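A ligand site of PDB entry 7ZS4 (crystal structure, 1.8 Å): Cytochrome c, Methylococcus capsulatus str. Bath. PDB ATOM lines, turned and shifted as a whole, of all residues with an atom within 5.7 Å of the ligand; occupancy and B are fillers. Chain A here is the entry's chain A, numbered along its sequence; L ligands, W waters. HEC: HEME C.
The backbone NH (N) of Met 104 is in hydrogen-bond range of the backbone carbonyl oxygen (O) of Leu 79, at 2.9 Å.
O of Glu 120 sits at hydrogen-bond distance from N of Val 103, 2.8 Å away.
N of His 56 is in hydrogen-bond range of O of Met 40, 2.9 Å away.
The side-chain carboxylate of Glu 120 lies within hydrogen-bond range of the backbone NH of Val 132 (3.0 Å).
ND1 of His 143 lies within hydrogen-bond range of O of Tyr 151 (2.8 Å).
The backbone carbonyl oxygen (O) of Lys 38 is in hydrogen-bond range of the backbone NH (N) of Val 58 (2.8 Å).
The backbone carbonyl oxygen (O) of Phe 81 sits at hydrogen-bond distance from the backbone NH (N) of Gly 102, at 2.7 Å.
A ring nitrogen (NE2) of His 143 is bound to an iron atom (FE) of the ligand, at 2.0 Å.
The side-chain sulfur (SG) of Cys 142 is covalently linked to a carbon (CAC) of the ligand (1.8 Å).
The backbone NH of Phe 153 lies within hydrogen-bond range of an oxygen (O2A) of the ligand, 2.9 Å away.
SG of Cys 139 is bonded to CAB of the ligand (1.8 Å).
The side-chain hydroxyl (OG) of Ser 154 sits at hydrogen-bond distance from an oxygen (O1A) of the ligand (2.6 Å).
An oxygen (O1A) of the ligand lies within hydrogen-bond range of the backbone NH (N) of Ser 154 (2.7 Å).
NZ of Lys 38 lies within salt-bridge range of O2D of the ligand.
NE2 of His 56 is in hydrogen-bond range of O1D of the ligand, 2.5 Å away.
Met 40 touches the ligand.
CG1 of Val 58 touches CAA of the ligand, 3.9 Å away.
Leu 79 touches the ligand.
Phe 81 touches the ligand.
O of Gly 102 touches CMA of the ligand (3.7 Å).
Val 103 touches the ligand (O to CMB, 3.8 Å).
SD of Met 104 touches C3A of the ligand, 3.7 Å away.
CB of Tyr 119 touches CMB of the ligand, at 3.9 Å.
Glu 120 touches the ligand.
CG2 of Val 132 touches CBB of the ligand (3.7 Å).
Val 152 touches the ligand (CA to O2A, 3.3 Å).
Hydrophobic or aromatic side chains within 4 Å of the ligand: Met 40, His 56, Val 58, Leu 79, Phe 81, Met 104, Tyr 119, Val 132, His 143, Val 152 and Phe 153.
Along chain A the residues within 4 Å of the ligand span positions 38 to 154.
The nearest printed residue that does not touch the ligand is Gly 138 (4.004 Å).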
ATOM      1  N   LYS A  38     -32.218 -36.321 -11.804  1.00  0.00           N
ATOM      2  CA  LYS A  38     -30.968 -37.086 -11.600  1.00  0.00           C
ATOM      3  C   LYS A  38     -30.222 -36.486 -10.426  1.00  0.00           C
ATOM      4  O   LYS A  38     -30.618 -35.383  -9.891  1.00  0.00           O
ATOM      5  CB  LYS A  38     -30.097 -37.056 -12.860  1.00  0.00           C
ATOM      6  CG  LYS A  38     -29.520 -35.684 -13.171  1.00  0.00           C
ATOM      7  CD  LYS A  38     -28.456 -35.680 -14.215  1.00  0.00           C
ATOM      8  CE  LYS A  38     -27.235 -36.467 -13.810  1.00  0.00           C
ATOM      9  NZ  LYS A  38     -26.186 -36.258 -14.821  1.00  0.00           N
ATOM     10  N   SER A  39     -29.161 -37.182 -10.033  1.00  0.00           N
ATOM     11  CA  SER A  39     -28.239 -36.745  -8.971  1.00  0.00           C
ATOM     12  C   SER A  39     -26.813 -37.077  -9.405  1.00  0.00           C
ATOM     13  O   SER A  39     -26.617 -37.947 -10.292  1.00  0.00           O
ATOM     14  CB  SER A  39     -28.559 -37.365  -7.657  1.00  0.00           C
ATOM     15  OG  SER A  39     -29.892 -37.073  -7.264  1.00  0.00           O
ATOM     16  N   MET A  40     -25.855 -36.460  -8.717  1.00  0.00           N
ATOM     17  CA  MET A  40     -24.407 -36.730  -8.877  1.00  0.00           C
ATOM     18  C   MET A  40     -23.702 -36.239  -7.593  1.00  0.00           C
ATOM     19  O   MET A  40     -24.224 -35.298  -6.937  1.00  0.00           O
ATOM     20  CB  MET A  40     -23.888 -35.994 -10.106  1.00  0.00           C
ATOM     21  CG  MET A  40     -22.428 -36.319 -10.464  1.00  0.00           C
ATOM     22  SD  MET A  40     -21.792 -35.239 -11.781  1.00  0.00           S
ATOM     23  CE  MET A  40     -22.840 -35.750 -13.146  1.00  0.00           C
ATOM     24  N   LEU A  48     -14.348 -29.311 -10.426  1.00  0.00           N
ATOM     25  CA  LEU A  48     -15.445 -28.377 -10.039  1.00  0.00           C
ATOM     26  C   LEU A  48     -15.790 -28.472  -8.540  1.00  0.00           C
ATOM     27  O   LEU A  48     -16.859 -27.922  -8.164  1.00  0.00           O
ATOM     28  CB  LEU A  48     -16.647 -28.680 -10.933  1.00  0.00           C
ATOM     29  CG  LEU A  48     -16.405 -28.619 -12.449  1.00  0.00           C
ATOM     30  CD1 LEU A  48     -17.704 -28.787 -13.225  1.00  0.00           C
ATOM     31  CD2 LEU A  48     -15.713 -27.322 -12.848  1.00  0.00           C
ATOM     32  N   HIS A  56     -25.497 -33.142  -5.477  1.00  0.00           N
ATOM     33  CA  HIS A  56     -26.519 -32.314  -6.139  1.00  0.00           C
ATOM     34  C   HIS A  56     -27.632 -33.173  -6.729  1.00  0.00           C
ATOM     35  O   HIS A  56     -27.367 -34.327  -7.163  1.00  0.00           O
ATOM     36  CB  HIS A  56     -25.931 -31.339  -7.158  1.00  0.00           C
ATOM     37  CG  HIS A  56     -25.440 -31.927  -8.421  1.00  0.00           C
ATOM     38  ND1 HIS A  56     -24.101 -32.085  -8.669  1.00  0.00           N
ATOM     39  CD2 HIS A  56     -26.077 -32.274  -9.560  1.00  0.00           C
ATOM     40  CE1 HIS A  56     -23.929 -32.516  -9.904  1.00  0.00           C
ATOM     41  NE2 HIS A  56     -25.131 -32.675 -10.443  1.00  0.00           N
ATOM     42  N   VAL A  58     -30.955 -32.599  -9.441  1.00  0.00           N
ATOM     43  CA  VAL A  58     -31.565 -31.767 -10.497  1.00  0.00           C
ATOM     44  C   VAL A  58     -33.079 -31.997 -10.449  1.00  0.00           C
ATOM     45  O   VAL A  58     -33.510 -33.153 -10.410  1.00  0.00           O
ATOM     46  CB  VAL A  58     -30.980 -32.086 -11.869  1.00  0.00           C
ATOM     47  CG1 VAL A  58     -31.611 -31.223 -12.943  1.00  0.00           C
ATOM     48  CG2 VAL A  58     -29.460 -31.966 -11.854  1.00  0.00           C
ATOM     49  N   LEU A  79     -35.311 -25.439 -14.540  1.00  0.00           N
ATOM     50  CA  LEU A  79     -34.411 -26.506 -14.023  1.00  0.00           C
ATOM     51  C   LEU A  79     -33.706 -25.971 -12.770  1.00  0.00           C
ATOM     52  O   LEU A  79     -33.319 -24.772 -12.760  1.00  0.00           O
ATOM     53  CB  LEU A  79     -33.430 -26.892 -15.106  1.00  0.00           C
ATOM     54  CG  LEU A  79     -34.067 -27.583 -16.318  1.00  0.00           C
ATOM     55  CD1 LEU A  79     -33.160 -27.482 -17.510  1.00  0.00           C
ATOM     56  CD2 LEU A  79     -34.358 -29.026 -16.002  1.00  0.00           C
ATOM     57  N   VAL A  80     -33.641 -26.797 -11.727  1.00  0.00           N
ATOM     58  CA  VAL A  80     -32.957 -26.410 -10.474  1.00  0.00           C
ATOM     59  C   VAL A  80     -31.835 -27.416 -10.206  1.00  0.00           C
ATOM     60  O   VAL A  80     -32.100 -28.632 -10.204  1.00  0.00           O
ATOM     61  CB  VAL A  80     -33.910 -26.324  -9.272  1.00  0.00           C
ATOM     62  CG1 VAL A  80     -33.144 -25.957  -8.002  1.00  0.00           C
ATOM     63  CG2 VAL A  80     -35.040 -25.346  -9.523  1.00  0.00           C
ATOM     64  N   PHE A  81     -30.647 -26.894  -9.938  1.00  0.00           N
ATOM     65  CA  PHE A  81     -29.475 -27.626  -9.421  1.00  0.00           C
ATOM     66  C   PHE A  81     -29.406 -27.376  -7.914  1.00  0.00           C
ATOM     67  O   PHE A  81     -29.104 -26.240  -7.533  1.00  0.00           O
ATOM     68  CB  PHE A  81     -28.231 -27.092 -10.132  1.00  0.00           C
ATOM     69  CG  PHE A  81     -26.910 -27.755  -9.805  1.00  0.00           C
ATOM     70  CD1 PHE A  81     -26.204 -27.427  -8.652  1.00  0.00           C
ATOM     71  CD2 PHE A  81     -26.324 -28.631 -10.712  1.00  0.00           C
ATOM     72  CE1 PHE A  81     -24.923 -27.953  -8.431  1.00  0.00           C
ATOM     73  CE2 PHE A  81     -25.060 -29.170 -10.487  1.00  0.00           C
ATOM     74  CZ  PHE A  81     -24.360 -28.835  -9.336  1.00  0.00           C
ATOM     75  N   GLY A 102     -28.705 -23.617  -8.162  1.00  0.00           N
ATOM     76  CA  GLY A 102     -28.648 -22.943  -9.462  1.00  0.00           C
ATOM     77  C   GLY A 102     -29.976 -23.099 -10.153  1.00  0.00           C
ATOM     78  O   GLY A 102     -30.650 -24.111  -9.921  1.00  0.00           O
ATOM     79  N   VAL A 103     -30.337 -22.112 -10.979  1.00  0.00           N
ATOM     80  CA  VAL A 103     -31.683 -22.015 -11.595  1.00  0.00           C
ATOM     81  C   VAL A 103     -31.499 -21.605 -13.048  1.00  0.00           C
ATOM     82  O   VAL A 103     -30.766 -20.609 -13.324  1.00  0.00           O
ATOM     83  CB  VAL A 103     -32.636 -21.076 -10.828  1.00  0.00           C
ATOM     84  CG1 VAL A 103     -34.040 -21.112 -11.383  1.00  0.00           C
ATOM     85  CG2 VAL A 103     -32.650 -21.436  -9.355  1.00  0.00           C
ATOM     86  N   MET A 104     -32.135 -22.378 -13.922  1.00  0.00           N
ATOM     87  CA  MET A 104     -32.280 -22.002 -15.345  1.00  0.00           C
ATOM     88  C   MET A 104     -33.768 -21.826 -15.627  1.00  0.00           C
ATOM     89  O   MET A 104     -34.547 -22.722 -15.323  1.00  0.00           O
ATOM     90  CB  MET A 104     -31.664 -23.065 -16.257  1.00  0.00           C
ATOM     91  CG  MET A 104     -30.161 -23.028 -16.261  1.00  0.00           C
ATOM     92  SD  MET A 104     -29.528 -24.584 -17.010  1.00  0.00           S
ATOM     93  CE  MET A 104     -29.959 -24.277 -18.728  1.00  0.00           C
ATOM     94  N   TYR A 119     -30.002 -17.487 -16.125  1.00  0.00           N
ATOM     95  CA  TYR A 119     -29.150 -18.212 -15.149  1.00  0.00           C
ATOM     96  C   TYR A 119     -29.073 -17.406 -13.837  1.00  0.00           C
ATOM     97  O   TYR A 119     -28.707 -16.260 -13.868  1.00  0.00           O
ATOM     98  CB  TYR A 119     -27.755 -18.427 -15.740  1.00  0.00           C
ATOM     99  CG  TYR A 119     -27.727 -19.354 -16.933  1.00  0.00           C
ATOM    100  CD1 TYR A 119     -27.926 -18.881 -18.224  1.00  0.00           C
ATOM    101  CD2 TYR A 119     -27.440 -20.704 -16.780  1.00  0.00           C
ATOM    102  CE1 TYR A 119     -27.871 -19.722 -19.320  1.00  0.00           C
ATOM    103  CE2 TYR A 119     -27.400 -21.552 -17.860  1.00  0.00           C
ATOM    104  CZ  TYR A 119     -27.617 -21.064 -19.136  1.00  0.00           C
ATOM    105  OH  TYR A 119     -27.601 -21.882 -20.225  1.00  0.00           O
ATOM    106  N   GLU A 120     -29.375 -18.046 -12.708  1.00  0.00           N
ATOM    107  CA  GLU A 120     -29.277 -17.399 -11.371  1.00  0.00           C
ATOM    108  C   GLU A 120     -28.838 -18.458 -10.360  1.00  0.00           C
ATOM    109  O   GLU A 120     -29.137 -19.639 -10.571  1.00  0.00           O
ATOM    110  CB  GLU A 120     -30.608 -16.775 -10.959  1.00  0.00           C
ATOM    111  CG  GLU A 120     -30.575 -16.104  -9.581  1.00  0.00           C
ATOM    112  CD  GLU A 120     -29.674 -14.879  -9.589  1.00  0.00           C
ATOM    113  OE1 GLU A 120     -30.180 -13.764  -9.826  1.00  0.00           O
ATOM    114  OE2 GLU A 120     -28.468 -15.068  -9.451  1.00  0.00           O
ATOM    115  N   GLY A 121     -28.202 -18.000  -9.293  1.00  0.00           N
ATOM    116  CA  GLY A 121     -27.823 -18.778  -8.126  1.00  0.00           C
ATOM    117  C   GLY A 121     -28.418 -18.152  -6.899  1.00  0.00           C
ATOM    118  O   GLY A 121     -28.523 -16.918  -6.852  1.00  0.00           O
ATOM    119  N   VAL A 132     -25.577 -14.261  -9.045  1.00  0.00           N
ATOM    120  CA  VAL A 132     -25.052 -13.987 -10.412  1.00  0.00           C
ATOM    121  C   VAL A 132     -24.920 -12.482 -10.602  1.00  0.00           C
ATOM    122  O   VAL A 132     -25.896 -11.772 -10.295  1.00  0.00           O
ATOM    123  CB  VAL A 132     -25.903 -14.640 -11.519  1.00  0.00           C
ATOM    124  CG1 VAL A 132     -25.626 -14.028 -12.880  1.00  0.00           C
ATOM    125  CG2 VAL A 132     -25.698 -16.160 -11.517  1.00  0.00           C
ATOM    126  N   GLY A 138     -21.113 -15.912 -17.627  1.00  0.00           N
ATOM    127  CA  GLY A 138     -20.262 -17.010 -17.128  1.00  0.00           C
ATOM    128  C   GLY A 138     -20.965 -18.368 -17.180  1.00  0.00           C
ATOM    129  O   GLY A 138     -20.405 -19.334 -17.696  1.00  0.00           O
ATOM    130  N   CYS A 139     -22.188 -18.453 -16.663  1.00  0.00           N
ATOM    131  CA  CYS A 139     -22.993 -19.699 -16.675  1.00  0.00           C
ATOM    132  C   CYS A 139     -23.132 -20.173 -18.128  1.00  0.00           C
ATOM    133  O   CYS A 139     -22.797 -21.374 -18.454  1.00  0.00           O
ATOM    134  CB  CYS A 139     -24.379 -19.455 -16.101  1.00  0.00           C
ATOM    135  SG  CYS A 139     -24.329 -18.742 -14.461  1.00  0.00           S
ATOM    136  N   CYS A 142     -20.275 -21.940 -20.191  1.00  0.00           N
ATOM    137  CA  CYS A 142     -20.103 -23.401 -20.061  1.00  0.00           C
ATOM    138  C   CYS A 142     -21.281 -24.131 -20.713  1.00  0.00           C
ATOM    139  O   CYS A 142     -21.045 -25.095 -21.482  1.00  0.00           O
ATOM    140  CB  CYS A 142     -19.885 -23.749 -18.601  1.00  0.00           C
ATOM    141  SG  CYS A 142     -19.442 -25.424 -18.422  1.00  0.00           S
ATOM    142  N   HIS A 143     -22.519 -23.697 -20.464  1.00  0.00           N
ATOM    143  CA  HIS A 143     -23.739 -24.382 -20.960  1.00  0.00           C
ATOM    144  C   HIS A 143     -23.806 -24.339 -22.502  1.00  0.00           C
ATOM    145  O   HIS A 143     -24.499 -25.201 -23.090  1.00  0.00           O
ATOM    146  CB  HIS A 143     -24.989 -23.836 -20.245  1.00  0.00           C
ATOM    147  CG  HIS A 143     -25.183 -24.419 -18.874  1.00  0.00           C
ATOM    148  ND1 HIS A 143     -26.162 -25.354 -18.610  1.00  0.00           N
ATOM    149  CD2 HIS A 143     -24.508 -24.232 -17.715  1.00  0.00           C
ATOM    150  CE1 HIS A 143     -26.083 -25.726 -17.317  1.00  0.00           C
ATOM    151  NE2 HIS A 143     -25.086 -25.042 -16.742  1.00  0.00           N
ATOM    152  N   TYR A 151     -28.888 -26.380 -24.295  1.00  0.00           N
ATOM    153  CA  TYR A 151     -28.019 -25.790 -23.236  1.00  0.00           C
ATOM    154  C   TYR A 151     -28.204 -26.520 -21.908  1.00  0.00           C
ATOM    155  O   TYR A 151     -27.741 -25.963 -20.879  1.00  0.00           O
ATOM    156  CB  TYR A 151     -28.323 -24.306 -23.073  1.00  0.00           C
ATOM    157  CG  TYR A 151     -28.078 -23.541 -24.346  1.00  0.00           C
ATOM    158  CD1 TYR A 151     -26.797 -23.384 -24.819  1.00  0.00           C
ATOM    159  CD2 TYR A 151     -29.127 -23.074 -25.112  1.00  0.00           C
ATOM    160  CE1 TYR A 151     -26.535 -22.696 -25.993  1.00  0.00           C
ATOM    161  CE2 TYR A 151     -28.902 -22.391 -26.289  1.00  0.00           C
ATOM    162  CZ  TYR A 151     -27.586 -22.182 -26.717  1.00  0.00           C
ATOM    163  OH  TYR A 151     -27.338 -21.501 -27.874  1.00  0.00           O
ATOM    164  N   VAL A 152     -28.782 -27.733 -21.933  1.00  0.00           N
ATOM    165  CA  VAL A 152     -29.068 -28.563 -20.729  1.00  0.00           C
ATOM    166  C   VAL A 152     -28.128 -29.761 -20.743  1.00  0.00           C
ATOM    167  O   VAL A 152     -28.052 -30.451 -21.775  1.00  0.00           O
ATOM    168  CB  VAL A 152     -30.536 -28.975 -20.669  1.00  0.00           C
ATOM    169  CG1 VAL A 152     -30.812 -29.890 -19.474  1.00  0.00           C
ATOM    170  CG2 VAL A 152     -31.435 -27.752 -20.640  1.00  0.00           C
ATOM    171  N   PHE A 153     -27.384 -29.958 -19.665  1.00  0.00           N
ATOM    172  CA  PHE A 153     -26.450 -31.101 -19.499  1.00  0.00           C
ATOM    173  C   PHE A 153     -27.237 -32.334 -19.110  1.00  0.00           C
ATOM    174  O   PHE A 153     -27.013 -33.408 -19.663  1.00  0.00           O
ATOM    175  CB  PHE A 153     -25.412 -30.802 -18.419  1.00  0.00           C
ATOM    176  CG  PHE A 153     -24.289 -29.912 -18.845  1.00  0.00           C
ATOM    177  CD1 PHE A 153     -24.334 -28.537 -18.592  1.00  0.00           C
ATOM    178  CD2 PHE A 153     -23.190 -30.413 -19.527  1.00  0.00           C
ATOM    179  CE1 PHE A 153     -23.309 -27.705 -18.990  1.00  0.00           C
ATOM    180  CE2 PHE A 153     -22.146 -29.589 -19.919  1.00  0.00           C
ATOM    181  CZ  PHE A 153     -22.194 -28.223 -19.636  1.00  0.00           C
ATOM    182  N   SER A 154     -28.130 -32.205 -18.130  1.00  0.00           N
ATOM    183  CA  SER A 154     -28.816 -33.333 -17.448  1.00  0.00           C
ATOM    184  C   SER A 154     -29.630 -34.120 -18.481  1.00  0.00           C
ATOM    185  O   SER A 154     -30.278 -33.487 -19.334  1.00  0.00           O
ATOM    186  CB  SER A 154     -29.708 -32.828 -16.330  1.00  0.00           C
ATOM    187  OG  SER A 154     -28.944 -32.353 -15.238  1.00  0.00           O
HETATM  188 FE   HEC L   1     -24.500 -25.385 -14.831  1.00  0.00          FE
HETATM  189  CHA HEC L   1     -26.146 -28.366 -14.667  1.00  0.00           C
HETATM  190  CHB HEC L   1     -27.182 -23.780 -13.581  1.00  0.00           C
HETATM  191  CHC HEC L   1     -22.576 -22.708 -14.309  1.00  0.00           C
HETATM  192  CHD HEC L   1     -21.800 -27.096 -15.951  1.00  0.00           C
HETATM  193  NA  HEC L   1     -26.350 -25.987 -14.127  1.00  0.00           N
HETATM  194  C1A HEC L   1     -26.897 -27.231 -14.269  1.00  0.00           C
HETATM  195  C2A HEC L   1     -28.295 -27.197 -14.013  1.00  0.00           C
HETATM  196  C3A HEC L   1     -28.595 -25.872 -13.672  1.00  0.00           C
HETATM  197  C4A HEC L   1     -27.376 -25.176 -13.782  1.00  0.00           C
HETATM  198  CMA HEC L   1     -29.949 -25.343 -13.303  1.00  0.00           C
HETATM  199  CAA HEC L   1     -29.283 -28.292 -14.192  1.00  0.00           C
HETATM  200  CBA HEC L   1     -29.718 -28.303 -15.665  1.00  0.00           C
HETATM  201  CGA HEC L   1     -28.683 -28.949 -16.608  1.00  0.00           C
HETATM  202  O1A HEC L   1     -28.309 -30.124 -16.399  1.00  0.00           O
HETATM  203  O2A HEC L   1     -28.182 -28.236 -17.515  1.00  0.00           O
HETATM  204  NB  HEC L   1     -24.853 -23.477 -14.143  1.00  0.00           N
HETATM  205  C1B HEC L   1     -26.014 -23.001 -13.717  1.00  0.00           C
HETATM  206  C2B HEC L   1     -25.871 -21.620 -13.312  1.00  0.00           C
HETATM  207  C3B HEC L   1     -24.518 -21.270 -13.510  1.00  0.00           C
HETATM  208  C4B HEC L   1     -23.964 -22.499 -14.013  1.00  0.00           C
HETATM  209  CMB HEC L   1     -26.965 -20.780 -12.746  1.00  0.00           C
HETATM  210  CAB HEC L   1     -23.784 -19.946 -13.278  1.00  0.00           C
HETATM  211  CBB HEC L   1     -23.951 -19.361 -11.867  1.00  0.00           C
HETATM  212  NC  HEC L   1     -22.576 -24.997 -15.080  1.00  0.00           N
HETATM  213  C1C HEC L   1     -21.972 -23.793 -14.918  1.00  0.00           C
HETATM  214  C2C HEC L   1     -20.639 -23.766 -15.440  1.00  0.00           C
HETATM  215  C3C HEC L   1     -20.389 -25.071 -15.957  1.00  0.00           C
HETATM  216  C4C HEC L   1     -21.596 -25.755 -15.684  1.00  0.00           C
HETATM  217  CMC HEC L   1     -19.783 -22.547 -15.389  1.00  0.00           C
HETATM  218  CAC HEC L   1     -19.183 -25.669 -16.689  1.00  0.00           C
HETATM  219  CBC HEC L   1     -17.846 -25.081 -16.271  1.00  0.00           C
HETATM  220  ND  HEC L   1     -23.995 -27.403 -15.107  1.00  0.00           N
HETATM  221  C1D HEC L   1     -22.840 -27.907 -15.525  1.00  0.00           C
HETATM  222  C2D HEC L   1     -22.841 -29.312 -15.551  1.00  0.00           C
HETATM  223  C3D HEC L   1     -24.120 -29.698 -15.168  1.00  0.00           C
HETATM  224  C4D HEC L   1     -24.788 -28.483 -14.918  1.00  0.00           C
HETATM  225  CMD HEC L   1     -21.703 -30.234 -15.965  1.00  0.00           C
HETATM  226  CAD HEC L   1     -24.686 -31.100 -15.108  1.00  0.00           C
HETATM  227  CBD HEC L   1     -24.688 -31.714 -13.691  1.00  0.00           C
HETATM  228  CGD HEC L   1     -25.199 -33.151 -13.730  1.00  0.00           C
HETATM  229  O1D HEC L   1     -25.521 -33.694 -12.669  1.00  0.00           O
HETATM  230  O2D HEC L   1     -25.212 -33.810 -14.824  1.00  0.00           O
HETATM  231  O   HOH W   1     -23.745 -34.054 -17.260  1.00  0.00           O
